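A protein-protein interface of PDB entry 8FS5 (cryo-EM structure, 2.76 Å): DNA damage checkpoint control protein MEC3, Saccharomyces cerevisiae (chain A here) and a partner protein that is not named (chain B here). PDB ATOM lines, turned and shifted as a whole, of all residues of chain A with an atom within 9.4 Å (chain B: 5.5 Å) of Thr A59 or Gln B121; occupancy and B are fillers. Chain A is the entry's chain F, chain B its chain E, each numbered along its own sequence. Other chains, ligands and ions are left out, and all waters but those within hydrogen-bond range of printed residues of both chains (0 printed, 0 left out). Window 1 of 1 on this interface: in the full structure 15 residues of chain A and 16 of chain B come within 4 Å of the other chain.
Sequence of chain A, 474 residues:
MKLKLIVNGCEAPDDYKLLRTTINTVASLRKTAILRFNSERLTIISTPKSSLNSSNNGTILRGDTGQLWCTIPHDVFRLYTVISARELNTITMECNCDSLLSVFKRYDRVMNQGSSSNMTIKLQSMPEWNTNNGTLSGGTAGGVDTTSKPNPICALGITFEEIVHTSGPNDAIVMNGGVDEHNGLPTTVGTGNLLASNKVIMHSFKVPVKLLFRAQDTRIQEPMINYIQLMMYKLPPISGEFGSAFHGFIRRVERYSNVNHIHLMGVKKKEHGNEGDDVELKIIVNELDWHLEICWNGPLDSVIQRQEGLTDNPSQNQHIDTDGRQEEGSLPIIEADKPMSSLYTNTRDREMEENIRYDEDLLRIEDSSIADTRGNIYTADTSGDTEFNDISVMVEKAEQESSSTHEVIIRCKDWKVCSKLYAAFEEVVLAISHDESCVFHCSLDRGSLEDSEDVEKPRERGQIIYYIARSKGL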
ATOM      1  N   ARG A  30      -6.169  -5.296   2.071  1.00  0.00           N
ATOM      2  CA  ARG A  30      -4.754  -4.963   2.004  1.00  0.00           C
ATOM      3  C   ARG A  30      -3.953  -5.967   2.817  1.00  0.00           C
ATOM      4  O   ARG A  30      -4.503  -6.758   3.589  1.00  0.00           O
ATOM      5  CB  ARG A  30      -4.482  -3.537   2.506  1.00  0.00           C
ATOM      6  CG  ARG A  30      -4.784  -3.328   3.979  1.00  0.00           C
ATOM      7  CD  ARG A  30      -4.768  -1.851   4.344  1.00  0.00           C
ATOM      8  NE  ARG A  30      -5.480  -1.034   3.369  1.00  0.00           N
ATOM      9  CZ  ARG A  30      -6.777  -0.762   3.421  1.00  0.00           C
ATOM     10  NH1 ARG A  30      -7.542  -1.229   4.395  1.00  0.00           N
ATOM     11  NH2 ARG A  30      -7.320  -0.003   2.474  1.00  0.00           N
ATOM     12  N   THR A  47      -6.322  -0.268   8.079  1.00  0.00           N
ATOM     13  CA  THR A  47      -6.246   1.154   7.769  1.00  0.00           C
ATOM     14  C   THR A  47      -4.937   1.485   7.064  1.00  0.00           C
ATOM     15  O   THR A  47      -3.871   1.003   7.473  1.00  0.00           O
ATOM     16  CB  THR A  47      -6.363   2.019   9.033  1.00  0.00           C
ATOM     17  OG1 THR A  47      -5.492   1.506  10.051  1.00  0.00           O
ATOM     18  CG2 THR A  47      -7.790   2.032   9.549  1.00  0.00           C
ATOM     19  N   PRO A  48      -4.990   2.292   5.999  1.00  0.00           N
ATOM     20  CA  PRO A  48      -3.747   2.782   5.386  1.00  0.00           C
ATOM     21  C   PRO A  48      -3.075   3.891   6.176  1.00  0.00           C
ATOM     22  O   PRO A  48      -1.886   4.153   5.948  1.00  0.00           O
ATOM     23  CB  PRO A  48      -4.213   3.288   4.016  1.00  0.00           C
ATOM     24  CG  PRO A  48      -5.617   3.730   4.266  1.00  0.00           C
ATOM     25  CD  PRO A  48      -6.183   2.749   5.264  1.00  0.00           C
ATOM     26  N   LYS A  49      -3.796   4.550   7.088  1.00  0.00           N
ATOM     27  CA  LYS A  49      -3.193   5.600   7.906  1.00  0.00           C
ATOM     28  C   LYS A  49      -2.189   5.019   8.896  1.00  0.00           C
ATOM     29  O   LYS A  49      -1.327   5.739   9.416  1.00  0.00           O
ATOM     30  CB  LYS A  49      -4.288   6.373   8.645  1.00  0.00           C
ATOM     31  CG  LYS A  49      -3.825   7.665   9.309  1.00  0.00           C
ATOM     32  CD  LYS A  49      -4.985   8.430   9.938  1.00  0.00           C
ATOM     33  CE  LYS A  49      -6.182   8.531   9.004  1.00  0.00           C
ATOM     34  NZ  LYS A  49      -5.827   9.145   7.694  1.00  0.00           N
ATOM     35  N   SER A  50      -2.290   3.718   9.176  1.00  0.00           N
ATOM     36  CA  SER A  50      -1.386   3.036  10.138  1.00  0.00           C
ATOM     37  C   SER A  50      -1.177   1.580   9.723  1.00  0.00           C
ATOM     38  O   SER A  50      -1.084   1.352   8.506  1.00  0.00           O
ATOM     39  CB  SER A  50      -1.929   3.133  11.537  1.00  0.00           C
ATOM     40  OG  SER A  50      -0.980   2.658  12.482  1.00  0.00           O
ATOM     41  N   SER A  54       1.674  -2.054   7.008  1.00  0.00           N
ATOM     42  CA  SER A  54       0.669  -1.946   5.916  1.00  0.00           C
ATOM     43  C   SER A  54       0.565  -0.478   5.506  1.00  0.00           C
ATOM     44  O   SER A  54      -0.391  -0.143   4.782  1.00  0.00           O
ATOM     45  CB  SER A  54      -0.680  -2.493   6.301  1.00  0.00           C
ATOM     46  OG  SER A  54      -1.392  -2.919   5.150  1.00  0.00           O
ATOM     47  N   SER A  55       1.505   0.362   5.945  1.00  0.00           N
ATOM     48  CA  SER A  55       1.510   1.815   5.634  1.00  0.00           C
ATOM     49  C   SER A  55       2.705   2.139   4.739  1.00  0.00           C
ATOM     50  O   SER A  55       3.406   3.122   5.038  1.00  0.00           O
ATOM     51  CB  SER A  55       1.523   2.640   6.895  1.00  0.00           C
ATOM     52  OG  SER A  55       2.555   2.212   7.771  1.00  0.00           O
ATOM     53  N   ASN A  56       2.932   1.348   3.686  1.00  0.00           N
ATOM     54  CA  ASN A  56       4.071   1.552   2.800  1.00  0.00           C
ATOM     55  C   ASN A  56       3.735   2.522   1.673  1.00  0.00           C
ATOM     56  O   ASN A  56       4.300   3.618   1.605  1.00  0.00           O
ATOM     57  CB  ASN A  56       4.531   0.210   2.225  1.00  0.00           C
ATOM     58  CG  ASN A  56       6.015   0.183   1.919  1.00  0.00           C
ATOM     59  OD1 ASN A  56       6.814   0.817   2.609  1.00  0.00           O
ATOM     60  ND2 ASN A  56       6.392  -0.554   0.882  1.00  0.00           N
ATOM     61  N   ASN A  57       2.809   2.134   0.785  1.00  0.00           N
ATOM     62  CA  ASN A  57       2.396   2.969  -0.346  1.00  0.00           C
ATOM     63  C   ASN A  57       0.879   2.857  -0.544  1.00  0.00           C
ATOM     64  O   ASN A  57       0.393   2.684  -1.665  1.00  0.00           O
ATOM     65  CB  ASN A  57       3.163   2.610  -1.618  1.00  0.00           C
ATOM     66  CG  ASN A  57       4.207   3.654  -1.980  1.00  0.00           C
ATOM     67  OD1 ASN A  57       4.770   4.312  -1.107  1.00  0.00           O
ATOM     68  ND2 ASN A  57       4.456   3.818  -3.273  1.00  0.00           N
ATOM     69  N   GLY A  58       0.129   2.955   0.553  1.00  0.00           N
ATOM     70  CA  GLY A  58      -1.315   2.823   0.480  1.00  0.00           C
ATOM     71  C   GLY A  58      -2.044   3.952  -0.227  1.00  0.00           C
ATOM     72  O   GLY A  58      -2.516   3.770  -1.353  1.00  0.00           O
ATOM     73  N   THR A  59      -2.147   5.119   0.411  1.00  0.00           N
ATOM     74  CA  THR A  59      -2.812   6.258  -0.218  1.00  0.00           C
ATOM     75  C   THR A  59      -1.795   7.148  -0.915  1.00  0.00           C
ATOM     76  O   THR A  59      -1.799   8.375  -0.758  1.00  0.00           O
ATOM     77  CB  THR A  59      -3.608   7.057   0.815  1.00  0.00           C
ATOM     78  OG1 THR A  59      -3.948   8.340   0.272  1.00  0.00           O
ATOM     79  CG2 THR A  59      -2.806   7.231   2.103  1.00  0.00           C
ATOM     80  N   ILE A  60      -0.932   6.517  -1.705  1.00  0.00           N
ATOM     81  CA  ILE A  60       0.226   7.140  -2.329  1.00  0.00           C
ATOM     82  C   ILE A  60       0.291   6.859  -3.829  1.00  0.00           C
ATOM     83  O   ILE A  60       0.477   7.787  -4.623  1.00  0.00           O
ATOM     84  CB  ILE A  60       1.506   6.736  -1.563  1.00  0.00           C
ATOM     85  CG1 ILE A  60       1.357   7.114  -0.071  1.00  0.00           C
ATOM     86  CG2 ILE A  60       2.761   7.263  -2.225  1.00  0.00           C
ATOM     87  CD1 ILE A  60       1.467   6.015   0.935  1.00  0.00           C
ATOM     88  N   LEU A  61       0.131   5.600  -4.245  1.00  0.00           N
ATOM     89  CA  LEU A  61       0.120   5.291  -5.673  1.00  0.00           C
ATOM     90  C   LEU A  61      -1.078   4.457  -6.121  1.00  0.00           C
ATOM     91  O   LEU A  61      -1.166   4.110  -7.306  1.00  0.00           O
ATOM     92  CB  LEU A  61       1.422   4.593  -6.074  1.00  0.00           C
ATOM     93  CG  LEU A  61       2.411   5.495  -6.814  1.00  0.00           C
ATOM     94  CD1 LEU A  61       3.676   4.730  -7.158  1.00  0.00           C
ATOM     95  CD2 LEU A  61       1.769   6.084  -8.061  1.00  0.00           C
ATOM     96  N   ARG A  62      -2.004   4.125  -5.221  1.00  0.00           N
ATOM     97  CA  ARG A  62      -3.178   3.347  -5.595  1.00  0.00           C
ATOM     98  C   ARG A  62      -4.495   3.941  -5.123  1.00  0.00           C
ATOM     99  O   ARG A  62      -5.551   3.411  -5.491  1.00  0.00           O
ATOM    100  CB  ARG A  62      -3.066   1.908  -5.064  1.00  0.00           C
ATOM    101  CG  ARG A  62      -1.883   1.140  -5.625  1.00  0.00           C
ATOM    102  CD  ARG A  62      -1.585  -0.109  -4.815  1.00  0.00           C
ATOM    103  NE  ARG A  62      -0.818   0.184  -3.611  1.00  0.00           N
ATOM    104  CZ  ARG A  62       0.463  -0.116  -3.449  1.00  0.00           C
ATOM    105  NH1 ARG A  62       1.161  -0.707  -4.406  1.00  0.00           N
ATOM    106  NH2 ARG A  62       1.060   0.183  -2.299  1.00  0.00           N
ATOM    107  N   GLY A  63      -4.474   5.011  -4.333  1.00  0.00           N
ATOM    108  CA  GLY A  63      -5.701   5.608  -3.843  1.00  0.00           C
ATOM    109  C   GLY A  63      -6.433   4.764  -2.826  1.00  0.00           C
ATOM    110  O   GLY A  63      -7.652   4.901  -2.680  1.00  0.00           O
ATOM    111  N   ASP A  64      -5.722   3.885  -2.124  1.00  0.00           N
ATOM    112  CA  ASP A  64      -6.326   2.997  -1.133  1.00  0.00           C
ATOM    113  C   ASP A  64      -6.477   3.769   0.171  1.00  0.00           C
ATOM    114  O   ASP A  64      -5.556   3.849   0.986  1.00  0.00           O
ATOM    115  CB  ASP A  64      -5.482   1.742  -0.947  1.00  0.00           C
ATOM    116  CG  ASP A  64      -5.422   0.889  -2.199  1.00  0.00           C
ATOM    117  OD1 ASP A  64      -6.071   1.258  -3.201  1.00  0.00           O
ATOM    118  OD2 ASP A  64      -4.722  -0.146  -2.185  1.00  0.00           O
ATOM    119  N   THR A  65      -7.659   4.353   0.367  1.00  0.00           N
ATOM    120  CA  THR A  65      -7.980   5.094   1.583  1.00  0.00           C
ATOM    121  C   THR A  65      -9.072   4.406   2.393  1.00  0.00           C
ATOM    122  O   THR A  65      -9.573   4.980   3.366  1.00  0.00           O
ATOM    123  CB  THR A  65      -8.399   6.527   1.248  1.00  0.00           C
ATOM    124  OG1 THR A  65      -9.596   6.505   0.460  1.00  0.00           O
ATOM    125  CG2 THR A  65      -7.302   7.237   0.471  1.00  0.00           C
ATOM    126  N   GLY A  66      -9.454   3.190   2.009  1.00  0.00           N
ATOM    127  CA  GLY A  66     -10.523   2.487   2.697  1.00  0.00           C
ATOM    128  C   GLY A  66     -10.095   2.034   4.081  1.00  0.00           C
ATOM    129  O   GLY A  66      -9.023   1.445   4.252  1.00  0.00           O
ATOM    130  N   GLN A  67     -10.940   2.305   5.073  1.00  0.00           N
ATOM    131  CA  GLN A  67     -10.675   1.950   6.465  1.00  0.00           C
ATOM    132  C   GLN A  67     -11.823   1.084   6.974  1.00  0.00           C
ATOM    133  O   GLN A  67     -12.964   1.546   7.071  1.00  0.00           O
ATOM    134  CB  GLN A  67     -10.502   3.200   7.325  1.00  0.00           C
ATOM    135  CG  GLN A  67      -9.468   4.180   6.797  1.00  0.00           C
ATOM    136  CD  GLN A  67      -9.208   5.324   7.757  1.00  0.00           C
ATOM    137  OE1 GLN A  67      -9.360   5.177   8.969  1.00  0.00           O
ATOM    138  NE2 GLN A  67      -8.813   6.471   7.218  1.00  0.00           N
ATOM    139  N   ALA A 469     -13.905   6.676   1.009  1.00  0.00           N
ATOM    140  CA  ALA A 469     -13.848   8.132   0.735  1.00  0.00           C
ATOM    141  C   ALA A 469     -14.186   8.408  -0.733  1.00  0.00           C
ATOM    142  O   ALA A 469     -13.968   7.519  -1.572  1.00  0.00           O
ATOM    143  CB  ALA A 469     -12.490   8.676   1.095  1.00  0.00           C
ATOM    144  N   ARG A 470     -14.689   9.607  -1.026  1.00  0.00           N
ATOM    145  CA  ARG A 470     -14.984   9.990  -2.431  1.00  0.00           C
ATOM    146  C   ARG A 470     -13.727   9.792  -3.279  1.00  0.00           C
ATOM    147  O   ARG A 470     -12.631  10.122  -2.794  1.00  0.00           O
ATOM    148  CB  ARG A 470     -15.442  11.448  -2.493  1.00  0.00           C
ATOM    149  CG  ARG A 470     -14.608  12.396  -1.644  1.00  0.00           C
ATOM    150  CD  ARG A 470     -13.723  13.298  -2.478  1.00  0.00           C
ATOM    151  NE  ARG A 470     -14.500  14.297  -3.193  1.00  0.00           N
ATOM    152  CZ  ARG A 470     -14.346  15.606  -3.046  1.00  0.00           C
ATOM    153  NH1 ARG A 470     -13.360  16.073  -2.303  1.00  0.00           N
ATOM    154  NH2 ARG A 470     -15.177  16.444  -3.643  1.00  0.00           N
ATOM    155  N   SER A 471     -13.883   9.268  -4.496  1.00  0.00           N
ATOM    156  CA  SER A 471     -12.727   9.074  -5.408  1.00  0.00           C
ATOM    157  C   SER A 471     -12.639  10.264  -6.364  1.00  0.00           C
ATOM    158  O   SER A 471     -11.560  10.466  -6.943  1.00  0.00           O
ATOM    159  CB  SER A 471     -12.845   7.779  -6.155  1.00  0.00           C
ATOM    160  OG  SER A 471     -11.702   7.563  -6.965  1.00  0.00           O
ATOM    161  N   LYS A 472     -13.733  11.013  -6.513  1.00  0.00           N
ATOM    162  CA  LYS A 472     -13.757  12.201  -7.406  1.00  0.00           C
ATOM    163  C   LYS A 472     -14.757  13.212  -6.852  1.00  0.00           C
ATOM    164  O   LYS A 472     -15.479  12.863  -5.902  1.00  0.00           O
ATOM    165  CB  LYS A 472     -14.205  11.819  -8.819  1.00  0.00           C
ATOM    166  CG  LYS A 472     -13.246  10.951  -9.620  1.00  0.00           C
ATOM    167  CD  LYS A 472     -13.879  10.417 -10.883  1.00  0.00           C
ATOM    168  CE  LYS A 472     -14.622  11.478 -11.665  1.00  0.00           C
ATOM    169  NZ  LYS A 472     -15.280  10.910 -12.866  1.00  0.00           N
ATOM    170  N   PRO B  91       5.912   7.938   1.069  1.00  0.00           N
ATOM    171  CA  PRO B  91       4.527   8.207   1.497  1.00  0.00           C
ATOM    172  C   PRO B  91       4.072   9.648   1.303  1.00  0.00           C
ATOM    173  O   PRO B  91       2.876   9.921   1.468  1.00  0.00           O
ATOM    174  CB  PRO B  91       4.537   7.828   2.988  1.00  0.00           C
ATOM    175  CG  PRO B  91       5.992   7.702   3.361  1.00  0.00           C
ATOM    176  CD  PRO B  91       6.672   7.242   2.118  1.00  0.00           C
ATOM    177  N   MET B 119      -5.753  12.014  -9.085  1.00  0.00           N
ATOM    178  CA  MET B 119      -6.137  11.586  -7.748  1.00  0.00           C
ATOM    179  C   MET B 119      -6.023  12.752  -6.776  1.00  0.00           C
ATOM    180  O   MET B 119      -4.979  13.403  -6.683  1.00  0.00           O
ATOM    181  CB  MET B 119      -5.257  10.420  -7.291  1.00  0.00           C
ATOM    182  CG  MET B 119      -5.316   9.205  -8.203  1.00  0.00           C
ATOM    183  SD  MET B 119      -5.441   7.651  -7.295  1.00  0.00           S
ATOM    184  CE  MET B 119      -3.711   7.251  -7.065  1.00  0.00           C
ATOM    185  N   GLU B 120      -7.109  13.011  -6.049  1.00  0.00           N
ATOM    186  CA  GLU B 120      -7.187  14.174  -5.176  1.00  0.00           C
ATOM    187  C   GLU B 120      -6.408  14.000  -3.878  1.00  0.00           C
ATOM    188  O   GLU B 120      -6.132  15.001  -3.207  1.00  0.00           O
ATOM    189  CB  GLU B 120      -8.656  14.487  -4.868  1.00  0.00           C
ATOM    190  CG  GLU B 120      -8.913  15.877  -4.304  1.00  0.00           C
ATOM    191  CD  GLU B 120     -10.372  16.105  -3.961  1.00  0.00           C
ATOM    192  OE1 GLU B 120     -11.166  15.146  -4.065  1.00  0.00           O
ATOM    193  OE2 GLU B 120     -10.724  17.243  -3.586  1.00  0.00           O
ATOM    194  N   GLN B 121      -6.029  12.768  -3.530  1.00  0.00           N
ATOM    195  CA  GLN B 121      -5.397  12.455  -2.247  1.00  0.00           C
ATOM    196  C   GLN B 121      -6.267  12.944  -1.090  1.00  0.00           C
ATOM    197  O   GLN B 121      -5.830  13.694  -0.215  1.00  0.00           O
ATOM    198  CB  GLN B 121      -3.982  13.038  -2.164  1.00  0.00           C
ATOM    199  CG  GLN B 121      -2.887  12.006  -1.923  1.00  0.00           C
ATOM    200  CD  GLN B 121      -2.742  11.619  -0.461  1.00  0.00           C
ATOM    201  OE1 GLN B 121      -3.584  11.955   0.372  1.00  0.00           O
ATOM    202  NE2 GLN B 121      -1.666  10.910  -0.144  1.00  0.00           N
ATOM    203  N   VAL B 122      -7.529  12.512  -1.108  1.00  0.00           N
ATOM    204  CA  VAL B 122      -8.500  12.965  -0.119  1.00  0.00           C
ATOM    205  C   VAL B 122      -8.155  12.460   1.282  1.00  0.00           C
ATOM    206  O   VAL B 122      -8.282  13.211   2.258  1.00  0.00           O
ATOM    207  CB  VAL B 122      -9.917  12.547  -0.554  1.00  0.00           C
ATOM    208  CG1 VAL B 122      -9.978  11.057  -0.869  1.00  0.00           C
ATOM    209  CG2 VAL B 122     -10.940  12.914   0.505  1.00  0.00           C
ATOM    210  N   ASP B 123      -7.703  11.215   1.400  1.00  0.00           N
ATOM    211  CA  ASP B 123      -7.340  10.572   2.679  1.00  0.00           C
ATOM    212  C   ASP B 123      -8.580  10.594   3.579  1.00  0.00           C
ATOM    213  O   ASP B 123      -9.709  10.491   3.076  1.00  0.00           O
ATOM    214  CB  ASP B 123      -6.104  11.236   3.261  1.00  0.00           C
ATOM    215  CG  ASP B 123      -5.362  10.340   4.233  1.00  0.00           C
ATOM    216  OD1 ASP B 123      -4.490   9.567   3.785  1.00  0.00           O
ATOM    217  OD2 ASP B 123      -5.651  10.409   5.447  1.00  0.00           O
ATOM    218  N   HIS B 133       0.010  16.101   3.050  1.00  0.00           N
ATOM    219  CA  HIS B 133      -0.842  14.979   2.652  1.00  0.00           C
ATOM    220  C   HIS B 133      -2.042  15.398   1.804  1.00  0.00           C
ATOM    221  O   HIS B 133      -2.833  14.544   1.393  1.00  0.00           O
ATOM    222  CB  HIS B 133      -1.302  14.164   3.877  1.00  0.00           C
ATOM    223  CG  HIS B 133      -2.435  14.775   4.645  1.00  0.00           C
ATOM    224  ND1 HIS B 133      -2.234  15.555   5.763  1.00  0.00           N
ATOM    225  CD2 HIS B 133      -3.775  14.715   4.463  1.00  0.00           C
ATOM    226  CE1 HIS B 133      -3.402  15.956   6.234  1.00  0.00           C
ATOM    227  NE2 HIS B 133      -4.353  15.459   5.463  1.00  0.00           N
ATOM    228  N   ARG B 134      -2.197  16.694   1.533  1.00  0.00           N
ATOM    229  CA  ARG B 134      -3.241  17.131   0.613  1.00  0.00           C
ATOM    230  C   ARG B 134      -2.713  17.195  -0.814  1.00  0.00           C
ATOM    231  O   ARG B 134      -3.216  16.497  -1.700  1.00  0.00           O
ATOM    232  CB  ARG B 134      -3.807  18.491   1.030  1.00  0.00           C
ATOM    233  CG  ARG B 134      -5.088  18.409   1.852  1.00  0.00           C
ATOM    234  CD  ARG B 134      -6.160  17.533   1.198  1.00  0.00           C
ATOM    235  NE  ARG B 134      -6.241  17.698  -0.250  1.00  0.00           N
ATOM    236  CZ  ARG B 134      -7.006  18.591  -0.863  1.00  0.00           C
ATOM    237  NH1 ARG B 134      -7.775  19.425  -0.183  1.00  0.00           N
ATOM    238  NH2 ARG B 134      -6.999  18.648  -2.192  1.00  0.00           N
ATOM    239  N   LYS B 136       0.636  16.802  -3.506  1.00  0.00           N
ATOM    240  CA  LYS B 136       1.707  15.833  -3.639  1.00  0.00           C
ATOM    241  C   LYS B 136       2.894  16.439  -4.374  1.00  0.00           C
ATOM    242  O   LYS B 136       2.737  17.297  -5.247  1.00  0.00           O
ATOM    243  CB  LYS B 136       1.210  14.591  -4.372  1.00  0.00           C
ATOM    244  CG  LYS B 136       0.712  13.514  -3.443  1.00  0.00           C
ATOM    245  CD  LYS B 136       1.037  12.169  -4.028  1.00  0.00           C
ATOM    246  CE  LYS B 136       1.159  11.120  -2.959  1.00  0.00           C
ATOM    247  NZ  LYS B 136       1.777   9.927  -3.556  1.00  0.00           N
ATOM    248  N   ASN B 164      -3.771  19.495  -6.173  1.00  0.00           N
ATOM    249  CA  ASN B 164      -3.465  18.192  -5.603  1.00  0.00           C
ATOM    250  C   ASN B 164      -2.074  17.683  -5.954  1.00  0.00           C
ATOM    251  O   ASN B 164      -1.731  16.560  -5.567  1.00  0.00           O
ATOM    252  CB  ASN B 164      -4.509  17.157  -6.045  1.00  0.00           C
ATOM    253  CG  ASN B 164      -4.918  17.322  -7.495  1.00  0.00           C
ATOM    254  OD1 ASN B 164      -5.029  18.440  -7.997  1.00  0.00           O
ATOM    255  ND2 ASN B 164      -5.147  16.205  -8.174  1.00  0.00           N
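OD2 of Asp B123 is in salt-bridge range of NZ of Lys A49 (2.6 Å).
The guanidinium group (NH1) of Arg A470 is in salt-bridge range of the side-chain carboxylate (OE1) of Glu B120 (3.0 Å).
The side-chain amino group (NZ) of Lys B136 sits at hydrogen-bond distance from the backbone carbonyl oxygen (O) of Ile A60, at 2.7 Å.
The side-chain amide nitrogen (NE2) of Gln B121 is in hydrogen-bond range of the backbone carbonyl oxygen (O) of Thr A59 (2.6 Å).
The backbone NH (N) of Lys B136 sits at hydrogen-bond distance from the backbone carbonyl oxygen (O) of Asn B164.
O of Asn A57 is in hydrogen-bond range of NH2 of Arg A62, at 2.7 Å.
The backbone carbonyl oxygen (O) of Met B119 lies within hydrogen-bond range of the side-chain amide nitrogen (ND2) of Asn B164 (3.2 Å).
The side-chain amide oxygen of Gln B121 sits close to the backbone carbonyl oxygen of His B133, at 2.9 Å.
O of Lys A472 lies within hydrogen-bond range of NE of Arg A470.
Thr A59 touches Asp B123 (CG2 to OD1, 3.3 Å).
CG1 of Ile A60 touches O of Pro B91, at 3.5 Å.
CE of Met B119 touches C of Leu A61, 3.95 Å away.
C of Arg A62 touches CE of Met B119, 3.9 Å away.
Met B119 touches Gly A63.
CG2 of Thr A65 touches CA of Asp B123, at 3.9999 Å.
CB of Ala A469 touches CG1 of Val B122, at 3.98 Å.
Asp B123 touches Ala A469 (O to CB, 3.9 Å).
O of Arg A470 touches CG1 of Val B122, 3.4 Å away.
Thr A59 touches just these residues of chain B: Gln B121 and Asp B123.
Gln B121 touches just one residue of chain A: Thr A59.
Of the printed residues of chain B, Gly A63 touches Met B119.
Of the printed residues of chain B, Arg A62 touches Met B119 (3.9 Å).
His B133 touches none of the printed residues of chain A.
The nearest printed residue of chain A that does not touch Asp B123 is Gln A67 (5.4 Å).
Of the 10 printed residues of chain B, 7 touch a printed residue of chain A.
Printed residues of chain B that touch a printed residue of chain A: Pro B91, Met B119, Glu B120, Gln B121, Val B122, Asp B123 and Lys B136.
Hydrophobic or aromatic side chains of chain B that line the printed part of chain A: Met B119 and Val B122.
Printed residues of chain A that touch a printed residue of chain B: Lys A49, Thr A59, Ile A60, Leu A61, Arg A62, Gly A63, Thr A65, Ala A469 and Arg A470.
Among the printed residues, Asp or Glu carboxylates within 4 Å of a Lys or Arg side-chain nitrogen of the other chain: Lys A49 with Asp B123 (2.6 Å) and Arg A470 with Glu B120 (3.0 Å).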
